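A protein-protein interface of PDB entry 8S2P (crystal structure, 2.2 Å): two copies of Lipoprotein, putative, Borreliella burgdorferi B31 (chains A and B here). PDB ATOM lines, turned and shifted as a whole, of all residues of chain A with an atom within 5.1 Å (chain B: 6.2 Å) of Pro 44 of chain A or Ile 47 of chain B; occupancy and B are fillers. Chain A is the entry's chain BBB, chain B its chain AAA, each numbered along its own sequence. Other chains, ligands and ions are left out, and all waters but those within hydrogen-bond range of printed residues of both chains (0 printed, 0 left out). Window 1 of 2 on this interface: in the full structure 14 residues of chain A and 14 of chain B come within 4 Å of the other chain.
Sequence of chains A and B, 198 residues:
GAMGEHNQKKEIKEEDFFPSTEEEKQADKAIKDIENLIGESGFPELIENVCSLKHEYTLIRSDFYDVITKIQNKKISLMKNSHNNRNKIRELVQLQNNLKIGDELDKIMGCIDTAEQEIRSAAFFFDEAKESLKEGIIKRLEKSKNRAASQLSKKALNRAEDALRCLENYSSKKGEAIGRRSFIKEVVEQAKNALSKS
OE1 of Glu 48 of chain A is in salt-bridge range of NH1 of Arg 120 of chain B, at 2.6 Å.
O of Ile 47 of chain B is in hydrogen-bond range of SG of Cys 51 of chain B, 3.7 Å away.
Pro 44 of chain A touches Ile 47 of chain B. Ile 47 of chain A touches Ile 47 of chain B (CG2 to CG2, 3.7 Å). Glu 48 of chain B touches Ile 47 of chain A.
Of chain B, only Ile 47 (3.9 Å) comes within 4 Å of Pro 44 of chain A. Printed residues of chain B within 4 Å of Ile 47 of chain A: Ile 47 (3.7 Å) and Glu 48 (3.9 Å). Printed residues of chain B within 4 Å of Glu 48 of chain A: Arg 120. Printed residues of chain A within 4 Å of Ile 47 of chain B: Pro 44 (3.9 Å) and Ile 47 (3.7 Å). Of the printed residues of chain A, Glu 48 of chain B touches Ile 47. Of the printed residues of chain A, Arg 120 of chain B touches Glu 48 (2.6 Å). The nearest residue of chain B that does not touch Pro 44 of chain A is Ala 123 of chain B (4.3 Å).
Of the 15 printed residues of chain B, 3 touch a printed residue of chain A. Hydrophobic or aromatic side chains of chain B that line the printed part of chain A: Ile 47. Hydrophobic or aromatic side chains of chain A that line the printed part of chain B: Pro 44 and Ile 47. Along chain A the printed residues that touch a printed residue of chain B span positions 44 to 48.
Pro 44 of chain A touches Ile 47 of chain B, but with the chains exchanged Ile 47 of chain A does not touch Pro 44 of chain B (4.1 Å). Ile 47 of chain B touches its own counterpart, Ile 47 of chain A. Ile 47 of chain A touches Glu 48 of chain B, but with the chains exchanged Glu 48 of chain A does not touch Ile 47 of chain B (4.2 Å). Of the 4 pairs that touch across the chains among the printed residues, 1 has its exchanged pair printed and touching as well.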
ATOM      1  N   SER A  41     -12.056   9.528   6.040  1.00  0.00           N
ATOM      2  CA  SER A  41     -12.179   8.359   5.133  1.00  0.00           C
ATOM      3  C   SER A  41     -13.472   8.517   4.319  1.00  0.00           C
ATOM      4  O   SER A  41     -13.629   7.828   3.321  1.00  0.00           O
ATOM      5  CB  SER A  41     -12.043   7.030   5.889  1.00  0.00           C
ATOM      6  OG  SER A  41     -12.918   6.938   7.008  1.00  0.00           O
ATOM      7  N   GLY A  42     -14.364   9.421   4.735  1.00  0.00           N
ATOM      8  CA  GLY A  42     -15.555   9.859   3.973  1.00  0.00           C
ATOM      9  C   GLY A  42     -16.506   8.722   3.627  1.00  0.00           C
ATOM     10  O   GLY A  42     -16.422   7.612   4.200  1.00  0.00           O
ATOM     11  N   PHE A  43     -17.388   8.978   2.679  1.00  0.00           N
ATOM     12  CA  PHE A  43     -18.439   8.025   2.272  1.00  0.00           C
ATOM     13  C   PHE A  43     -17.837   6.723   1.787  1.00  0.00           C
ATOM     14  O   PHE A  43     -18.416   5.676   2.080  1.00  0.00           O
ATOM     15  CB  PHE A  43     -19.400   8.711   1.305  1.00  0.00           C
ATOM     16  CG  PHE A  43     -20.442   9.477   2.082  1.00  0.00           C
ATOM     17  CD1 PHE A  43     -21.402   8.792   2.803  1.00  0.00           C
ATOM     18  CD2 PHE A  43     -20.435  10.859   2.138  1.00  0.00           C
ATOM     19  CE1 PHE A  43     -22.365   9.472   3.531  1.00  0.00           C
ATOM     20  CE2 PHE A  43     -21.402  11.531   2.865  1.00  0.00           C
ATOM     21  CZ  PHE A  43     -22.365  10.844   3.558  1.00  0.00           C
ATOM     22  N   PRO A  44     -16.715   6.745   1.035  1.00  0.00           N
ATOM     23  CA  PRO A  44     -16.080   5.513   0.546  1.00  0.00           C
ATOM     24  C   PRO A  44     -15.816   4.436   1.610  1.00  0.00           C
ATOM     25  O   PRO A  44     -16.141   3.291   1.353  1.00  0.00           O
ATOM     26  CB  PRO A  44     -14.777   6.022  -0.080  1.00  0.00           C
ATOM     27  CG  PRO A  44     -15.135   7.405  -0.567  1.00  0.00           C
ATOM     28  CD  PRO A  44     -16.070   7.951   0.491  1.00  0.00           C
ATOM     29  N   GLU A  45     -15.276   4.789   2.784  1.00  0.00           N
ATOM     30  CA  GLU A  45     -15.097   3.838   3.917  1.00  0.00           C
ATOM     31  C   GLU A  45     -16.482   3.297   4.319  1.00  0.00           C
ATOM     32  O   GLU A  45     -16.635   2.070   4.410  1.00  0.00           O
ATOM     33  CB  GLU A  45     -14.298   4.476   5.051  1.00  0.00           C
ATOM     34  CG  GLU A  45     -14.221   3.663   6.349  1.00  0.00           C
ATOM     35  CD  GLU A  45     -13.468   2.339   6.279  1.00  0.00           C
ATOM     36  OE1 GLU A  45     -13.173   1.886   5.169  1.00  0.00           O
ATOM     37  OE2 GLU A  45     -13.176   1.755   7.354  1.00  0.00           O
ATOM     38  N   LEU A  46     -17.484   4.159   4.445  1.00  0.00           N
ATOM     39  CA  LEU A  46     -18.834   3.747   4.906  1.00  0.00           C
ATOM     40  C   LEU A  46     -19.488   2.787   3.891  1.00  0.00           C
ATOM     41  O   LEU A  46     -20.109   1.827   4.365  1.00  0.00           O
ATOM     42  CB  LEU A  46     -19.658   4.997   5.220  1.00  0.00           C
ATOM     43  CG  LEU A  46     -19.090   5.832   6.369  1.00  0.00           C
ATOM     44  CD1 LEU A  46     -20.029   6.953   6.764  1.00  0.00           C
ATOM     45  CD2 LEU A  46     -18.768   4.967   7.584  1.00  0.00           C
ATOM     46  N   ILE A  47     -19.231   2.925   2.585  1.00  0.00           N
ATOM     47  CA  ILE A  47     -19.729   1.978   1.537  1.00  0.00           C
ATOM     48  C   ILE A  47     -19.026   0.619   1.698  1.00  0.00           C
ATOM     49  O   ILE A  47     -19.731  -0.387   1.891  1.00  0.00           O
ATOM     50  CB  ILE A  47     -19.603   2.585   0.121  1.00  0.00           C
ATOM     51  CG1 ILE A  47     -20.515   3.805  -0.023  1.00  0.00           C
ATOM     52  CG2 ILE A  47     -19.874   1.558  -0.960  1.00  0.00           C
ATOM     53  CD1 ILE A  47     -19.861   4.955  -0.731  1.00  0.00           C
ATOM     54  N   GLU A  48     -17.702   0.573   1.700  1.00  0.00           N
ATOM     55  CA  GLU A  48     -16.930  -0.675   1.972  1.00  0.00           C
ATOM     56  C   GLU A  48     -17.419  -1.372   3.257  1.00  0.00           C
ATOM     57  O   GLU A  48     -17.564  -2.596   3.230  1.00  0.00           O
ATOM     58  CB  GLU A  48     -15.431  -0.383   2.115  1.00  0.00           C
ATOM     59  CG  GLU A  48     -14.730  -0.039   0.815  1.00  0.00           C
ATOM     60  CD  GLU A  48     -13.346   0.584   1.034  1.00  0.00           C
ATOM     61  OE1 GLU A  48     -12.566   0.054   1.831  1.00  0.00           O
ATOM     62  OE2 GLU A  48     -13.060   1.616   0.447  1.00  0.00           O
ATOM     63  N   GLY B  42     -21.972   8.009  -9.701  1.00  0.00           N
ATOM     64  CA  GLY B  42     -20.774   8.599  -9.059  1.00  0.00           C
ATOM     65  C   GLY B  42     -19.872   7.543  -8.477  1.00  0.00           C
ATOM     66  O   GLY B  42     -19.942   6.391  -8.931  1.00  0.00           O
ATOM     67  N   PHE B  43     -19.026   7.906  -7.511  1.00  0.00           N
ATOM     68  CA  PHE B  43     -17.999   7.007  -6.920  1.00  0.00           C
ATOM     69  C   PHE B  43     -18.647   5.851  -6.151  1.00  0.00           C
ATOM     70  O   PHE B  43     -18.136   4.726  -6.207  1.00  0.00           O
ATOM     71  CB  PHE B  43     -16.971   7.813  -6.122  1.00  0.00           C
ATOM     72  CG  PHE B  43     -16.008   8.583  -6.990  1.00  0.00           C
ATOM     73  CD1 PHE B  43     -14.941   7.948  -7.583  1.00  0.00           C
ATOM     74  CD2 PHE B  43     -16.148   9.942  -7.202  1.00  0.00           C
ATOM     75  CE1 PHE B  43     -14.072   8.639  -8.410  1.00  0.00           C
ATOM     76  CE2 PHE B  43     -15.276  10.637  -8.031  1.00  0.00           C
ATOM     77  CZ  PHE B  43     -14.243   9.985  -8.638  1.00  0.00           C
ATOM     78  N   PRO B  44     -19.732   6.069  -5.372  1.00  0.00           N
ATOM     79  CA  PRO B  44     -20.465   4.968  -4.736  1.00  0.00           C
ATOM     80  C   PRO B  44     -20.695   3.723  -5.598  1.00  0.00           C
ATOM     81  O   PRO B  44     -20.277   2.661  -5.196  1.00  0.00           O
ATOM     82  CB  PRO B  44     -21.794   5.652  -4.364  1.00  0.00           C
ATOM     83  CG  PRO B  44     -21.343   7.022  -3.946  1.00  0.00           C
ATOM     84  CD  PRO B  44     -20.281   7.378  -4.968  1.00  0.00           C
ATOM     85  N   GLU B  45     -21.336   3.866  -6.751  1.00  0.00           N
ATOM     86  CA  GLU B  45     -21.488   2.757  -7.732  1.00  0.00           C
ATOM     87  C   GLU B  45     -20.130   2.100  -8.022  1.00  0.00           C
ATOM     88  O   GLU B  45     -20.039   0.868  -7.940  1.00  0.00           O
ATOM     89  CB  GLU B  45     -22.131   3.272  -9.015  1.00  0.00           C
ATOM     90  CG  GLU B  45     -22.277   2.231 -10.121  1.00  0.00           C
ATOM     91  CD  GLU B  45     -22.900   0.886  -9.774  1.00  0.00           C
ATOM     92  OE1 GLU B  45     -23.615   0.791  -8.744  1.00  0.00           O
ATOM     93  OE2 GLU B  45     -22.680  -0.074 -10.558  1.00  0.00           O
ATOM     94  N   LEU B  46     -19.109   2.881  -8.362  1.00  0.00           N
ATOM     95  CA  LEU B  46     -17.783   2.326  -8.779  1.00  0.00           C
ATOM     96  C   LEU B  46     -17.141   1.596  -7.594  1.00  0.00           C
ATOM     97  O   LEU B  46     -16.528   0.528  -7.853  1.00  0.00           O
ATOM     98  CB  LEU B  46     -16.908   3.437  -9.363  1.00  0.00           C
ATOM     99  CG  LEU B  46     -17.455   4.078 -10.652  1.00  0.00           C
ATOM    100  CD1 LEU B  46     -16.716   5.351 -11.002  1.00  0.00           C
ATOM    101  CD2 LEU B  46     -17.402   3.136 -11.869  1.00  0.00           C
ATOM    102  N   ILE B  47     -17.338   2.061  -6.345  1.00  0.00           N
ATOM    103  CA  ILE B  47     -16.792   1.368  -5.142  1.00  0.00           C
ATOM    104  C   ILE B  47     -17.535   0.048  -4.963  1.00  0.00           C
ATOM    105  O   ILE B  47     -16.888  -0.995  -4.849  1.00  0.00           O
ATOM    106  CB  ILE B  47     -16.862   2.243  -3.880  1.00  0.00           C
ATOM    107  CG1 ILE B  47     -15.897   3.418  -3.982  1.00  0.00           C
ATOM    108  CG2 ILE B  47     -16.588   1.423  -2.644  1.00  0.00           C
ATOM    109  CD1 ILE B  47     -16.384   4.648  -3.306  1.00  0.00           C
ATOM    110  N   GLU B  48     -18.859   0.083  -5.009  1.00  0.00           N
ATOM    111  CA  GLU B  48     -19.690  -1.149  -5.016  1.00  0.00           C
ATOM    112  C   GLU B  48     -19.238  -2.094  -6.137  1.00  0.00           C
ATOM    113  O   GLU B  48     -19.304  -3.321  -5.926  1.00  0.00           O
ATOM    114  CB  GLU B  48     -21.176  -0.810  -5.184  1.00  0.00           C
ATOM    115  CG  GLU B  48     -21.748  -0.059  -4.002  1.00  0.00           C
ATOM    116  CD  GLU B  48     -23.106   0.573  -4.231  1.00  0.00           C
ATOM    117  OE1 GLU B  48     -23.810   0.188  -5.183  1.00  0.00           O
ATOM    118  OE2 GLU B  48     -23.447   1.468  -3.463  1.00  0.00           O
ATOM    119  N   ASN B  49     -18.863  -1.581  -7.309  1.00  0.00           N
ATOM    120  CA  ASN B  49     -18.559  -2.460  -8.475  1.00  0.00           C
ATOM    121  C   ASN B  49     -17.359  -3.343  -8.117  1.00  0.00           C
ATOM    122  O   ASN B  49     -17.253  -4.475  -8.636  1.00  0.00           O
ATOM    123  CB  ASN B  49     -18.281  -1.681  -9.765  1.00  0.00           C
ATOM    124  CG  ASN B  49     -19.527  -1.185 -10.457  1.00  0.00           C
ATOM    125  OD1 ASN B  49     -20.599  -1.780 -10.338  1.00  0.00           O
ATOM    126  ND2 ASN B  49     -19.401  -0.088 -11.178  1.00  0.00           N
ATOM    127  N   VAL B  50     -16.471  -2.837  -7.266  1.00  0.00           N
ATOM    128  CA  VAL B  50     -15.249  -3.582  -6.855  1.00  0.00           C
ATOM    129  C   VAL B  50     -15.665  -4.663  -5.852  1.00  0.00           C
ATOM    130  O   VAL B  50     -15.313  -5.836  -6.084  1.00  0.00           O
ATOM    131  CB  VAL B  50     -14.169  -2.631  -6.314  1.00  0.00           C
ATOM    132  CG1 VAL B  50     -13.218  -3.319  -5.352  1.00  0.00           C
ATOM    133  CG2 VAL B  50     -13.408  -1.979  -7.459  1.00  0.00           C
ATOM    134  N   CYS B  51     -16.406  -4.272  -4.811  1.00  0.00           N
ATOM    135  CA  CYS B  51     -17.066  -5.166  -3.827  1.00  0.00           C
ATOM    136  C   CYS B  51     -17.753  -6.338  -4.555  1.00  0.00           C
ATOM    137  O   CYS B  51     -17.705  -7.478  -4.069  1.00  0.00           O
ATOM    138  CB  CYS B  51     -18.118  -4.394  -3.040  1.00  0.00           C
ATOM    139  SG  CYS B  51     -17.492  -3.125  -1.902  1.00  0.00           S
ATOM    140  N   SER B  52     -18.400  -6.063  -5.678  1.00  0.00           N
ATOM    141  CA  SER B  52     -19.238  -7.047  -6.392  1.00  0.00           C
ATOM    142  C   SER B  52     -18.321  -8.048  -7.091  1.00  0.00           C
ATOM    143  O   SER B  52     -18.662  -9.260  -7.136  1.00  0.00           O
ATOM    144  CB  SER B  52     -20.163  -6.364  -7.343  1.00  0.00           C
ATOM    145  OG  SER B  52     -21.454  -6.875  -7.159  1.00  0.00           O
ATOM    146  N   ILE B 119      -9.759   3.494  -6.965  1.00  0.00           N
ATOM    147  CA  ILE B 119     -11.054   4.225  -6.885  1.00  0.00           C
ATOM    148  C   ILE B 119     -11.079   5.055  -5.583  1.00  0.00           C
ATOM    149  O   ILE B 119     -11.564   6.181  -5.642  1.00  0.00           O
ATOM    150  CB  ILE B 119     -12.272   3.306  -7.067  1.00  0.00           C
ATOM    151  CG1 ILE B 119     -13.519   4.132  -7.384  1.00  0.00           C
ATOM    152  CG2 ILE B 119     -12.464   2.369  -5.878  1.00  0.00           C
ATOM    153  CD1 ILE B 119     -13.529   4.674  -8.812  1.00  0.00           C
ATOM    154  N   ARG B 120     -10.535   4.549  -4.467  1.00  0.00           N
ATOM    155  CA  ARG B 120     -10.458   5.328  -3.208  1.00  0.00           C
ATOM    156  C   ARG B 120      -9.678   6.609  -3.502  1.00  0.00           C
ATOM    157  O   ARG B 120     -10.213   7.672  -3.179  1.00  0.00           O
ATOM    158  CB  ARG B 120      -9.825   4.539  -2.058  1.00  0.00           C
ATOM    159  CG  ARG B 120     -10.711   3.452  -1.462  1.00  0.00           C
ATOM    160  CD  ARG B 120     -10.532   3.280   0.043  1.00  0.00           C
ATOM    161  NE  ARG B 120      -9.477   2.323   0.338  1.00  0.00           N
ATOM    162  CZ  ARG B 120      -9.613   0.998   0.328  1.00  0.00           C
ATOM    163  NH1 ARG B 120     -10.775   0.455   0.047  1.00  0.00           N
ATOM    164  NH2 ARG B 120      -8.583   0.211   0.594  1.00  0.00           N
ATOM    165  N   ALA B 123     -11.613   9.191  -5.852  1.00  0.00           N
ATOM    166  CA  ALA B 123     -12.625   9.897  -5.039  1.00  0.00           C
ATOM    167  C   ALA B 123     -11.948  11.031  -4.251  1.00  0.00           C
ATOM    168  O   ALA B 123     -12.455  12.156  -4.298  1.00  0.00           O
ATOM    169  CB  ALA B 123     -13.337   8.929  -4.115  1.00  0.00           C
ATOM    170  N   TYR B 170      -8.071   2.331 -12.628  1.00  0.00           N
ATOM    171  CA  TYR B 170      -9.211   1.559 -12.075  1.00  0.00           C
ATOM    172  C   TYR B 170      -9.885   0.751 -13.200  1.00  0.00           C
ATOM    173  O   TYR B 170     -10.056  -0.496 -13.113  1.00  0.00           O
ATOM    174  CB  TYR B 170     -10.184   2.514 -11.381  1.00  0.00           C
ATOM    175  CG  TYR B 170     -11.558   1.947 -11.168  1.00  0.00           C
ATOM    176  CD1 TYR B 170     -11.829   1.154 -10.069  1.00  0.00           C
ATOM    177  CD2 TYR B 170     -12.578   2.185 -12.083  1.00  0.00           C
ATOM    178  CE1 TYR B 170     -13.089   0.616  -9.870  1.00  0.00           C
ATOM    179  CE2 TYR B 170     -13.840   1.664 -11.894  1.00  0.00           C
ATOM    180  CZ  TYR B 170     -14.097   0.878 -10.776  1.00  0.00           C
ATOM    181  OH  TYR B 170     -15.348   0.368 -10.558  1.00  0.00           O
